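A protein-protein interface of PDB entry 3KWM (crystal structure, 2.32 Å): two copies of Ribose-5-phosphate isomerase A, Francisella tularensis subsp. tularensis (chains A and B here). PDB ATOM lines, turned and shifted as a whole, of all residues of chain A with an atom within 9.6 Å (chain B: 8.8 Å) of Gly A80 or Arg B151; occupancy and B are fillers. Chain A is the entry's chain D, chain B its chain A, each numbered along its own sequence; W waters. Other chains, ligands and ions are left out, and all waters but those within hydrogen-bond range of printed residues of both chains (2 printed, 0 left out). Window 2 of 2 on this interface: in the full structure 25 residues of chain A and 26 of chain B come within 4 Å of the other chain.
The side-chain amide oxygen (OD1) of Asn A77 lies within hydrogen-bond range of the side-chain hydroxyl (OG) of Ser B147, at 2.7 Å. The backbone carbonyl oxygen of Gly A80 sits at hydrogen-bond distance from the guanidinium group of Arg B151. OD1 of Asn A77 lies close to NH2 of Arg B146, at 3.5 Å.
The side-chain amide nitrogen (ND2) of Asn A77 lies within hydrogen-bond range of the side-chain carboxylate (OD2) of Asp A75, at 3.1 Å.
Among the printed residues, pairs that only touch across the chains: Leu A76 with Met B144, Asn A77 with Met B144, Ile A111 with Ala B145, Cys A112 with Met B144 and Ala A114 with Tyr B148.
Of the printed residues of chain B, Leu A76 touches Met B144 (3.7 Å). Of the printed residues of chain B, Asn A77 touches Met B144, Arg B146 and Ser B147. No residue of chain B comes within 4 Å of Ala A79. Gly A80 touches one residue of chain B. Printed residues of chain B within 4 Å of Ile A111: Ala B145 (3.6 Å). Of the printed residues of chain B, Ala A114 touches Tyr B148 (3.3 Å). Lys A117 touches none of the printed residues of chain B. Of the printed residues of chain A, Tyr B148 touches Ala A114. Ala B150 touches none of the printed residues of chain A. Of chain A, only Gly A80 (3.3 Å) comes within 4 Å of Arg B151. No residue of chain A comes within 4 Å of Val B154. Gly B158 touches none of the printed residues of chain A. The nearest residue of chain B that does not touch Gly A80 is Tyr B148 (5.7 Å). The nearest printed residue of chain B that does not touch Asn A77 is Ala B145 (4.7 Å).
Of the 19 printed residues of chain B, 6 touch a printed residue of chain A. Of the 21 printed residues of chain A, 6 touch a printed residue of chain B. Hydrophobic or aromatic side chains of chain A that line the printed part of chain B: Leu A76, Ile A111 and Ala A114. Among the printed residues, no Asp or Glu carboxylate lies within 4 Å of a Lys or Arg side-chain nitrogen of the other chain.
No position is printed for both chains.
Water W1 bridges the side-chain carboxylate (OD1) of Asp A75 (2.8 Å) and the backbone NH (N) of Met B144 (3.4 Å). Water W2 lies within hydrogen-bond range of the backbone NH of Leu A76 (2.8 Å) and the side-chain sulfur of Met B144 (3.7 Å).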
ATOM      1  N   THR A  29      26.003  30.133 -14.807  1.00  0.00           N
ATOM      2  CA  THR A  29      25.636  29.423 -16.026  1.00  0.00           C
ATOM      3  C   THR A  29      24.152  29.696 -16.239  1.00  0.00           C
ATOM      4  O   THR A  29      23.317  29.275 -15.440  1.00  0.00           O
ATOM      5  CB  THR A  29      25.868  27.903 -15.912  1.00  0.00           C
ATOM      6  OG1 THR A  29      27.253  27.649 -15.668  1.00  0.00           O
ATOM      7  CG2 THR A  29      25.451  27.191 -17.191  1.00  0.00           C
ATOM      8  N   THR A  54      28.497  31.441 -18.919  1.00  0.00           N
ATOM      9  CA  THR A  54      28.079  30.371 -19.811  1.00  0.00           C
ATOM     10  C   THR A  54      26.592  30.512 -20.131  1.00  0.00           C
ATOM     11  O   THR A  54      25.788  30.860 -19.261  1.00  0.00           O
ATOM     12  CB  THR A  54      28.332  28.990 -19.159  1.00  0.00           C
ATOM     13  OG1 THR A  54      29.556  29.022 -18.409  1.00  0.00           O
ATOM     14  CG2 THR A  54      28.426  27.902 -20.206  1.00  0.00           C
ATOM     15  N   VAL A  55      26.241  30.258 -21.389  1.00  0.00           N
ATOM     16  CA  VAL A  55      24.848  30.265 -21.829  1.00  0.00           C
ATOM     17  C   VAL A  55      24.489  28.914 -22.436  1.00  0.00           C
ATOM     18  O   VAL A  55      25.177  28.433 -23.339  1.00  0.00           O
ATOM     19  CB  VAL A  55      24.567  31.367 -22.887  1.00  0.00           C
ATOM     20  CG1 VAL A  55      23.085  31.419 -23.226  1.00  0.00           C
ATOM     21  CG2 VAL A  55      25.045  32.725 -22.407  1.00  0.00           C
ATOM     22  N   VAL A  56      23.417  28.311 -21.927  1.00  0.00           N
ATOM     23  CA  VAL A  56      22.839  27.105 -22.518  1.00  0.00           C
ATOM     24  C   VAL A  56      21.502  27.475 -23.157  1.00  0.00           C
ATOM     25  O   VAL A  56      20.703  28.198 -22.565  1.00  0.00           O
ATOM     26  CB  VAL A  56      22.648  25.980 -21.465  1.00  0.00           C
ATOM     27  CG1 VAL A  56      21.969  24.757 -22.078  1.00  0.00           C
ATOM     28  CG2 VAL A  56      23.986  25.588 -20.857  1.00  0.00           C
ATOM     29  N   VAL A  74      26.802  27.325 -25.166  1.00  0.00           N
ATOM     30  CA  VAL A  74      27.536  26.141 -24.751  1.00  0.00           C
ATOM     31  C   VAL A  74      26.581  24.954 -24.568  1.00  0.00           C
ATOM     32  O   VAL A  74      25.564  25.060 -23.878  1.00  0.00           O
ATOM     33  CB  VAL A  74      28.356  26.446 -23.464  1.00  0.00           C
ATOM     34  CG1 VAL A  74      28.678  25.195 -22.677  1.00  0.00           C
ATOM     35  CG2 VAL A  74      29.636  27.197 -23.808  1.00  0.00           C
ATOM     36  N   ASP A  75      26.912  23.840 -25.216  1.00  0.00           N
ATOM     37  CA  ASP A  75      26.172  22.584 -25.087  1.00  0.00           C
ATOM     38  C   ASP A  75      26.079  22.141 -23.624  1.00  0.00           C
ATOM     39  O   ASP A  75      27.064  22.220 -22.888  1.00  0.00           O
ATOM     40  CB  ASP A  75      26.847  21.496 -25.927  1.00  0.00           C
ATOM     41  CG  ASP A  75      26.053  20.208 -25.964  1.00  0.00           C
ATOM     42  OD1 ASP A  75      25.022  20.158 -26.666  1.00  0.00           O
ATOM     43  OD2 ASP A  75      26.462  19.241 -25.298  1.00  0.00           O
ATOM     44  N   LEU A  76      24.901  21.667 -23.216  1.00  0.00           N
ATOM     45  CA  LEU A  76      24.635  21.322 -21.815  1.00  0.00           C
ATOM     46  C   LEU A  76      25.569  20.256 -21.248  1.00  0.00           C
ATOM     47  O   LEU A  76      25.835  20.244 -20.048  1.00  0.00           O
ATOM     48  CB  LEU A  76      23.169  20.909 -21.613  1.00  0.00           C
ATOM     49  CG  LEU A  76      22.683  20.641 -20.175  1.00  0.00           C
ATOM     50  CD1 LEU A  76      22.863  21.860 -19.260  1.00  0.00           C
ATOM     51  CD2 LEU A  76      21.232  20.176 -20.165  1.00  0.00           C
ATOM     52  N   ASN A  77      26.061  19.373 -22.114  1.00  0.00           N
ATOM     53  CA  ASN A  77      26.955  18.289 -21.706  1.00  0.00           C
ATOM     54  C   ASN A  77      28.286  18.736 -21.101  1.00  0.00           C
ATOM     55  O   ASN A  77      28.778  18.107 -20.157  1.00  0.00           O
ATOM     56  CB  ASN A  77      27.190  17.322 -22.864  1.00  0.00           C
ATOM     57  CG  ASN A  77      26.010  16.412 -23.097  1.00  0.00           C
ATOM     58  OD1 ASN A  77      25.750  15.514 -22.305  1.00  0.00           O
ATOM     59  ND2 ASN A  77      25.287  16.640 -24.184  1.00  0.00           N
ATOM     60  N   TYR A  78      28.869  19.809 -21.639  1.00  0.00           N
ATOM     61  CA  TYR A  78      30.062  20.388 -21.015  1.00  0.00           C
ATOM     62  C   TYR A  78      29.796  21.610 -20.119  1.00  0.00           C
ATOM     63  O   TYR A  78      30.681  22.042 -19.389  1.00  0.00           O
ATOM     64  CB  TYR A  78      31.222  20.613 -22.012  1.00  0.00           C
ATOM     65  CG  TYR A  78      30.858  21.157 -23.380  1.00  0.00           C
ATOM     66  CD1 TYR A  78      30.225  22.386 -23.510  1.00  0.00           C
ATOM     67  CD2 TYR A  78      31.201  20.461 -24.552  1.00  0.00           C
ATOM     68  CE1 TYR A  78      29.904  22.909 -24.762  1.00  0.00           C
ATOM     69  CE2 TYR A  78      30.882  20.977 -25.824  1.00  0.00           C
ATOM     70  CZ  TYR A  78      30.229  22.210 -25.912  1.00  0.00           C
ATOM     71  OH  TYR A  78      29.884  22.763 -27.130  1.00  0.00           O
ATOM     72  N   ALA A  79      28.576  22.141 -20.148  1.00  0.00           N
ATOM     73  CA  ALA A  79      28.160  23.137 -19.155  1.00  0.00           C
ATOM     74  C   ALA A  79      27.871  22.478 -17.803  1.00  0.00           C
ATOM     75  O   ALA A  79      28.194  23.034 -16.750  1.00  0.00           O
ATOM     76  CB  ALA A  79      26.961  23.915 -19.635  1.00  0.00           C
ATOM     77  N   GLY A  80      27.260  21.295 -17.841  1.00  0.00           N
ATOM     78  CA  GLY A  80      27.029  20.490 -16.641  1.00  0.00           C
ATOM     79  C   GLY A  80      25.691  20.776 -15.990  1.00  0.00           C
ATOM     80  O   GLY A  80      24.709  20.048 -16.204  1.00  0.00           O
ATOM     81  N   GLU A  81      25.652  21.847 -15.202  1.00  0.00           N
ATOM     82  CA  GLU A  81      24.469  22.208 -14.437  1.00  0.00           C
ATOM     83  C   GLU A  81      24.148  23.678 -14.666  1.00  0.00           C
ATOM     84  O   GLU A  81      25.025  24.536 -14.567  1.00  0.00           O
ATOM     85  CB  GLU A  81      24.714  21.934 -12.950  1.00  0.00           C
ATOM     86  CG  GLU A  81      23.465  21.625 -12.130  1.00  0.00           C
ATOM     87  CD  GLU A  81      23.778  20.902 -10.816  1.00  0.00           C
ATOM     88  OE1 GLU A  81      24.790  20.166 -10.753  1.00  0.00           O
ATOM     89  OE2 GLU A  81      23.002  21.061  -9.843  1.00  0.00           O
ATOM     90  N   ILE A  82      22.893  23.966 -14.993  1.00  0.00           N
ATOM     91  CA  ILE A  82      22.446  25.346 -15.177  1.00  0.00           C
ATOM     92  C   ILE A  82      22.175  25.970 -13.804  1.00  0.00           C
ATOM     93  O   ILE A  82      21.533  25.348 -12.954  1.00  0.00           O
ATOM     94  CB  ILE A  82      21.195  25.417 -16.091  1.00  0.00           C
ATOM     95  CG1 ILE A  82      21.535  24.912 -17.498  1.00  0.00           C
ATOM     96  CG2 ILE A  82      20.627  26.836 -16.153  1.00  0.00           C
ATOM     97  CD1 ILE A  82      20.322  24.654 -18.386  1.00  0.00           C
ATOM     98  N   ASP A  83      22.692  27.179 -13.584  1.00  0.00           N
ATOM     99  CA  ASP A  83      22.428  27.919 -12.350  1.00  0.00           C
ATOM    100  C   ASP A  83      21.039  28.559 -12.372  1.00  0.00           C
ATOM    101  O   ASP A  83      20.270  28.430 -11.417  1.00  0.00           O
ATOM    102  CB  ASP A  83      23.493  28.996 -12.110  1.00  0.00           C
ATOM    103  CG  ASP A  83      24.856  28.415 -11.757  1.00  0.00           C
ATOM    104  OD1 ASP A  83      24.926  27.428 -10.995  1.00  0.00           O
ATOM    105  OD2 ASP A  83      25.870  28.965 -12.233  1.00  0.00           O
ATOM    106  N   ILE A 111      14.493  19.525 -20.538  1.00  0.00           N
ATOM    107  CA  ILE A 111      15.835  19.051 -20.204  1.00  0.00           C
ATOM    108  C   ILE A 111      16.607  20.135 -19.450  1.00  0.00           C
ATOM    109  O   ILE A 111      17.204  19.852 -18.413  1.00  0.00           O
ATOM    110  CB  ILE A 111      16.623  18.591 -21.470  1.00  0.00           C
ATOM    111  CG1 ILE A 111      16.010  17.308 -22.049  1.00  0.00           C
ATOM    112  CG2 ILE A 111      18.113  18.406 -21.152  1.00  0.00           C
ATOM    113  CD1 ILE A 111      16.477  16.962 -23.463  1.00  0.00           C
ATOM    114  N   CYS A 112      16.581  21.365 -19.970  1.00  0.00           N
ATOM    115  CA  CYS A 112      17.175  22.533 -19.288  1.00  0.00           C
ATOM    116  C   CYS A 112      16.642  22.743 -17.869  1.00  0.00           C
ATOM    117  O   CYS A 112      17.417  23.016 -16.957  1.00  0.00           O
ATOM    118  CB  CYS A 112      16.961  23.816 -20.098  1.00  0.00           C
ATOM    119  SG  CYS A 112      17.972  23.969 -21.580  1.00  0.00           S
ATOM    120  N   VAL A 113      15.326  22.624 -17.697  1.00  0.00           N
ATOM    121  CA  VAL A 113      14.688  22.724 -16.375  1.00  0.00           C
ATOM    122  C   VAL A 113      15.200  21.632 -15.429  1.00  0.00           C
ATOM    123  O   VAL A 113      15.581  21.923 -14.300  1.00  0.00           O
ATOM    124  CB  VAL A 113      13.116  22.693 -16.458  1.00  0.00           C
ATOM    125  CG1 VAL A 113      12.479  22.652 -15.062  1.00  0.00           C
ATOM    126  CG2 VAL A 113      12.591  23.892 -17.228  1.00  0.00           C
ATOM    127  N   ALA A 114      15.210  20.384 -15.897  1.00  0.00           N
ATOM    128  CA  ALA A 114      15.765  19.258 -15.134  1.00  0.00           C
ATOM    129  C   ALA A 114      17.188  19.528 -14.648  1.00  0.00           C
ATOM    130  O   ALA A 114      17.543  19.181 -13.519  1.00  0.00           O
ATOM    131  CB  ALA A 114      15.727  17.974 -15.972  1.00  0.00           C
ATOM    132  N   ALA A 115      17.994  20.158 -15.503  1.00  0.00           N
ATOM    133  CA  ALA A 115      19.403  20.414 -15.201  1.00  0.00           C
ATOM    134  C   ALA A 115      19.644  21.755 -14.510  1.00  0.00           C
ATOM    135  O   ALA A 115      20.797  22.129 -14.269  1.00  0.00           O
ATOM    136  CB  ALA A 115      20.239  20.311 -16.473  1.00  0.00           C
ATOM    137  N   ALA A 116      18.564  22.467 -14.181  1.00  0.00           N
ATOM    138  CA  ALA A 116      18.667  23.822 -13.613  1.00  0.00           C
ATOM    139  C   ALA A 116      18.445  23.863 -12.098  1.00  0.00           C
ATOM    140  O   ALA A 116      17.528  23.216 -11.575  1.00  0.00           O
ATOM    141  CB  ALA A 116      17.712  24.777 -14.316  1.00  0.00           C
ATOM    142  N   LYS A 117      19.296  24.626 -11.409  1.00  0.00           N
ATOM    143  CA  LYS A 117      19.197  24.822  -9.961  1.00  0.00           C
ATOM    144  C   LYS A 117      17.976  25.662  -9.596  1.00  0.00           C
ATOM    145  O   LYS A 117      17.299  25.378  -8.609  1.00  0.00           O
ATOM    146  CB  LYS A 117      20.460  25.488  -9.408  1.00  0.00           C
ATOM    147  CG  LYS A 117      21.705  24.614  -9.429  1.00  0.00           C
ATOM    148  CD  LYS A 117      22.777  25.197  -8.515  1.00  0.00           C
ATOM    149  CE  LYS A 117      24.086  24.423  -8.600  1.00  0.00           C
ATOM    150  NZ  LYS A 117      24.931  24.840  -9.763  1.00  0.00           N
ATOM    151  N   MET B 144      21.447  16.111 -25.871  1.00  0.00           N
ATOM    152  CA  MET B 144      21.610  17.223 -24.924  1.00  0.00           C
ATOM    153  C   MET B 144      21.465  16.831 -23.440  1.00  0.00           C
ATOM    154  O   MET B 144      22.003  17.506 -22.555  1.00  0.00           O
ATOM    155  CB  MET B 144      20.599  18.319 -25.276  1.00  0.00           C
ATOM    156  CG  MET B 144      20.489  19.433 -24.277  1.00  0.00           C
ATOM    157  SD  MET B 144      19.244  20.614 -24.785  1.00  0.00           S
ATOM    158  CE  MET B 144      19.554  21.905 -23.599  1.00  0.00           C
ATOM    159  N   ALA B 145      20.734  15.748 -23.181  1.00  0.00           N
ATOM    160  CA  ALA B 145      20.446  15.294 -21.817  1.00  0.00           C
ATOM    161  C   ALA B 145      21.338  14.134 -21.350  1.00  0.00           C
ATOM    162  O   ALA B 145      21.144  13.601 -20.259  1.00  0.00           O
ATOM    163  CB  ALA B 145      18.981  14.909 -21.702  1.00  0.00           C
ATOM    164  N   ARG B 146      22.315  13.754 -22.165  1.00  0.00           N
ATOM    165  CA  ARG B 146      23.116  12.552 -21.907  1.00  0.00           C
ATOM    166  C   ARG B 146      23.787  12.552 -20.526  1.00  0.00           C
ATOM    167  O   ARG B 146      23.691  11.575 -19.785  1.00  0.00           O
ATOM    168  CB  ARG B 146      24.158  12.348 -23.021  1.00  0.00           C
ATOM    169  CG  ARG B 146      25.253  11.346 -22.675  1.00  0.00           C
ATOM    170  CD  ARG B 146      26.272  11.181 -23.792  1.00  0.00           C
ATOM    171  NE  ARG B 146      26.778  12.443 -24.332  1.00  0.00           N
ATOM    172  CZ  ARG B 146      27.835  13.096 -23.859  1.00  0.00           C
ATOM    173  NH1 ARG B 146      28.509  12.620 -22.819  1.00  0.00           N
ATOM    174  NH2 ARG B 146      28.214  14.233 -24.425  1.00  0.00           N
ATOM    175  N   SER B 147      24.463  13.648 -20.198  1.00  0.00           N
ATOM    176  CA  SER B 147      25.210  13.767 -18.949  1.00  0.00           C
ATOM    177  C   SER B 147      24.286  13.842 -17.734  1.00  0.00           C
ATOM    178  O   SER B 147      24.542  13.195 -16.714  1.00  0.00           O
ATOM    179  CB  SER B 147      26.134  14.986 -18.994  1.00  0.00           C
ATOM    180  OG  SER B 147      27.051  14.890 -20.070  1.00  0.00           O
ATOM    181  N   TYR B 148      23.214  14.626 -17.850  1.00  0.00           N
ATOM    182  CA  TYR B 148      22.211  14.720 -16.793  1.00  0.00           C
ATOM    183  C   TYR B 148      21.623  13.338 -16.476  1.00  0.00           C
ATOM    184  O   TYR B 148      21.532  12.945 -15.313  1.00  0.00           O
ATOM    185  CB  TYR B 148      21.105  15.721 -17.160  1.00  0.00           C
ATOM    186  CG  TYR B 148      19.887  15.601 -16.268  1.00  0.00           C
ATOM    187  CD1 TYR B 148      19.830  16.251 -15.032  1.00  0.00           C
ATOM    188  CD2 TYR B 148      18.801  14.812 -16.651  1.00  0.00           C
ATOM    189  CE1 TYR B 148      18.715  16.120 -14.208  1.00  0.00           C
ATOM    190  CE2 TYR B 148      17.691  14.677 -15.843  1.00  0.00           C
ATOM    191  CZ  TYR B 148      17.652  15.324 -14.627  1.00  0.00           C
ATOM    192  OH  TYR B 148      16.538  15.176 -13.838  1.00  0.00           O
ATOM    193  N   ILE B 149      21.250  12.603 -17.520  1.00  0.00           N
ATOM    194  CA  ILE B 149      20.675  11.272 -17.368  1.00  0.00           C
ATOM    195  C   ILE B 149      21.644  10.258 -16.741  1.00  0.00           C
ATOM    196  O   ILE B 149      21.238   9.474 -15.868  1.00  0.00           O
ATOM    197  CB  ILE B 149      20.115  10.743 -18.709  1.00  0.00           C
ATOM    198  CG1 ILE B 149      18.980  11.654 -19.185  1.00  0.00           C
ATOM    199  CG2 ILE B 149      19.645   9.288 -18.565  1.00  0.00           C
ATOM    200  CD1 ILE B 149      18.604  11.458 -20.630  1.00  0.00           C
ATOM    201  N   ALA B 150      22.906  10.281 -17.180  1.00  0.00           N
ATOM    202  CA  ALA B 150      23.954   9.422 -16.607  1.00  0.00           C
ATOM    203  C   ALA B 150      24.069   9.618 -15.093  1.00  0.00           C
ATOM    204  O   ALA B 150      24.200   8.641 -14.341  1.00  0.00           O
ATOM    205  CB  ALA B 150      25.310   9.669 -17.291  1.00  0.00           C
ATOM    206  N   ARG B 151      24.006  10.878 -14.657  1.00  0.00           N
ATOM    207  CA  ARG B 151      24.036  11.209 -13.235  1.00  0.00           C
ATOM    208  C   ARG B 151      22.852  10.604 -12.475  1.00  0.00           C
ATOM    209  O   ARG B 151      23.035  10.090 -11.366  1.00  0.00           O
ATOM    210  CB  ARG B 151      24.089  12.727 -13.015  1.00  0.00           C
ATOM    211  CG  ARG B 151      25.417  13.376 -13.397  1.00  0.00           C
ATOM    212  CD  ARG B 151      25.591  14.770 -12.773  1.00  0.00           C
ATOM    213  NE  ARG B 151      24.574  15.739 -13.208  1.00  0.00           N
ATOM    214  CZ  ARG B 151      24.713  16.601 -14.220  1.00  0.00           C
ATOM    215  NH1 ARG B 151      25.834  16.628 -14.938  1.00  0.00           N
ATOM    216  NH2 ARG B 151      23.726  17.444 -14.517  1.00  0.00           N
ATOM    217  N   GLN B 152      21.655  10.659 -13.069  1.00  0.00           N
ATOM    218  CA  GLN B 152      20.434  10.137 -12.437  1.00  0.00           C
ATOM    219  C   GLN B 152      20.449   8.614 -12.323  1.00  0.00           C
ATOM    220  O   GLN B 152      19.871   8.049 -11.390  1.00  0.00           O
ATOM    221  CB  GLN B 152      19.169  10.587 -13.184  1.00  0.00           C
ATOM    222  CG  GLN B 152      18.958  12.104 -13.309  1.00  0.00           C
ATOM    223  CD  GLN B 152      19.093  12.852 -11.985  1.00  0.00           C
ATOM    224  OE1 GLN B 152      20.081  13.552 -11.756  1.00  0.00           O
ATOM    225  NE2 GLN B 152      18.103  12.702 -11.111  1.00  0.00           N
ATOM    226  N   ILE B 153      21.108   7.958 -13.279  1.00  0.00           N
ATOM    227  CA  ILE B 153      21.241   6.497 -13.292  1.00  0.00           C
ATOM    228  C   ILE B 153      22.217   6.028 -12.215  1.00  0.00           C
ATOM    229  O   ILE B 153      22.006   4.988 -11.588  1.00  0.00           O
ATOM    230  CB  ILE B 153      21.641   5.973 -14.708  1.00  0.00           C
ATOM    231  CG1 ILE B 153      20.460   6.121 -15.674  1.00  0.00           C
ATOM    232  CG2 ILE B 153      22.105   4.520 -14.665  1.00  0.00           C
ATOM    233  CD1 ILE B 153      20.851   6.025 -17.127  1.00  0.00           C
ATOM    234  N   VAL B 154      23.272   6.812 -11.996  1.00  0.00           N
ATOM    235  CA  VAL B 154      24.217   6.565 -10.906  1.00  0.00           C
ATOM    236  C   VAL B 154      23.474   6.538  -9.576  1.00  0.00           C
ATOM    237  O   VAL B 154      23.712   5.657  -8.740  1.00  0.00           O
ATOM    238  CB  VAL B 154      25.362   7.612 -10.887  1.00  0.00           C
ATOM    239  CG1 VAL B 154      26.133   7.575  -9.569  1.00  0.00           C
ATOM    240  CG2 VAL B 154      26.314   7.369 -12.047  1.00  0.00           C
ATOM    241  N   LYS B 155      22.555   7.494  -9.412  1.00  0.00           N
ATOM    242  CA  LYS B 155      21.715   7.607  -8.221  1.00  0.00           C
ATOM    243  C   LYS B 155      20.778   6.411  -8.064  1.00  0.00           C
ATOM    244  O   LYS B 155      20.385   6.074  -6.949  1.00  0.00           O
ATOM    245  CB  LYS B 155      20.900   8.903  -8.261  1.00  0.00           C
ATOM    246  CG  LYS B 155      21.733  10.178  -8.205  1.00  0.00           C
ATOM    247  CD  LYS B 155      20.844  11.404  -8.300  1.00  0.00           C
ATOM    248  CE  LYS B 155      21.642  12.694  -8.205  1.00  0.00           C
ATOM    249  NZ  LYS B 155      20.737  13.882  -8.127  1.00  0.00           N
ATOM    250  N   LEU B 156      20.416   5.783  -9.181  1.00  0.00           N
ATOM    251  CA  LEU B 156      19.598   4.570  -9.155  1.00  0.00           C
ATOM    252  C   LEU B 156      20.390   3.281  -8.879  1.00  0.00           C
ATOM    253  O   LEU B 156      19.799   2.209  -8.718  1.00  0.00           O
ATOM    254  CB  LEU B 156      18.790   4.435 -10.450  1.00  0.00           C
ATOM    255  CG  LEU B 156      17.534   5.308 -10.551  1.00  0.00           C
ATOM    256  CD1 LEU B 156      16.962   5.274 -11.959  1.00  0.00           C
ATOM    257  CD2 LEU B 156      16.473   4.904  -9.518  1.00  0.00           C
ATOM    258  N   GLY B 157      21.717   3.389  -8.829  1.00  0.00           N
ATOM    259  CA  GLY B 157      22.587   2.241  -8.554  1.00  0.00           C
ATOM    260  C   GLY B 157      23.262   1.623  -9.772  1.00  0.00           C
ATOM    261  O   GLY B 157      24.018   0.661  -9.646  1.00  0.00           O
ATOM    262  N   GLY B 158      22.999   2.172 -10.952  1.00  0.00           N
ATOM    263  CA  GLY B 158      23.569   1.632 -12.184  1.00  0.00           C
ATOM    264  C   GLY B 158      24.896   2.262 -12.554  1.00  0.00           C
ATOM    265  O   GLY B 158      25.277   3.300 -12.008  1.00  0.00           O
ATOM    266  N   GLN B 159      25.603   1.632 -13.486  1.00  0.00           N
ATOM    267  CA  GLN B 159      26.826   2.208 -14.043  1.00  0.00           C
ATOM    268  C   GLN B 159      26.624   2.569 -15.523  1.00  0.00           C
ATOM    269  O   GLN B 159      26.765   1.711 -16.406  1.00  0.00           O
ATOM    270  CB  GLN B 159      28.015   1.262 -13.858  1.00  0.00           C
ATOM    271  CG  GLN B 159      28.422   1.046 -12.403  1.00  0.00           C
ATOM    272  CD  GLN B 159      29.634   0.155 -12.270  1.00  0.00           C
ATOM    273  OE1 GLN B 159      29.592  -1.030 -12.615  1.00  0.00           O
ATOM    274  NE2 GLN B 159      30.730   0.721 -11.769  1.00  0.00           N
ATOM    275  N   PRO B 160      26.283   3.843 -15.796  1.00  0.00           N
ATOM    276  CA  PRO B 160      26.018   4.291 -17.165  1.00  0.00           C
ATOM    277  C   PRO B 160      27.286   4.459 -17.999  1.00  0.00           C
ATOM    278  O   PRO B 160      28.300   4.952 -17.505  1.00  0.00           O
ATOM    279  CB  PRO B 160      25.347   5.645 -16.953  1.00  0.00           C
ATOM    280  CG  PRO B 160      25.994   6.157 -15.690  1.00  0.00           C
ATOM    281  CD  PRO B 160      26.123   4.938 -14.822  1.00  0.00           C
ATOM    282  N   LEU B 175      22.881   5.253 -23.920  1.00  0.00           N
ATOM    283  CA  LEU B 175      23.576   4.921 -22.691  1.00  0.00           C
ATOM    284  C   LEU B 175      23.315   3.461 -22.347  1.00  0.00           C
ATOM    285  O   LEU B 175      22.160   3.023 -22.311  1.00  0.00           O
ATOM    286  CB  LEU B 175      23.102   5.804 -21.541  1.00  0.00           C
ATOM    287  CG  LEU B 175      23.481   7.284 -21.561  1.00  0.00           C
ATOM    288  CD1 LEU B 175      22.672   7.992 -20.497  1.00  0.00           C
ATOM    289  CD2 LEU B 175      24.977   7.500 -21.341  1.00  0.00           C
ATOM    290  N   ILE B 195      12.616   9.941 -16.232  1.00  0.00           N
ATOM    291  CA  ILE B 195      13.814  10.778 -16.350  1.00  0.00           C
ATOM    292  C   ILE B 195      13.738  11.635 -17.623  1.00  0.00           C
ATOM    293  O   ILE B 195      13.648  11.106 -18.731  1.00  0.00           O
ATOM    294  CB  ILE B 195      15.143   9.948 -16.318  1.00  0.00           C
ATOM    295  CG1 ILE B 195      15.248   9.099 -15.043  1.00  0.00           C
ATOM    296  CG2 ILE B 195      16.367  10.868 -16.436  1.00  0.00           C
ATOM    297  CD1 ILE B 195      16.308   7.992 -15.116  1.00  0.00           C
HETATM  298  O   HOH W   1      23.893  17.736 -27.503  1.00  0.00           O
HETATM  299  O   HOH W   2      22.589  22.083 -24.805  1.00  0.00           O
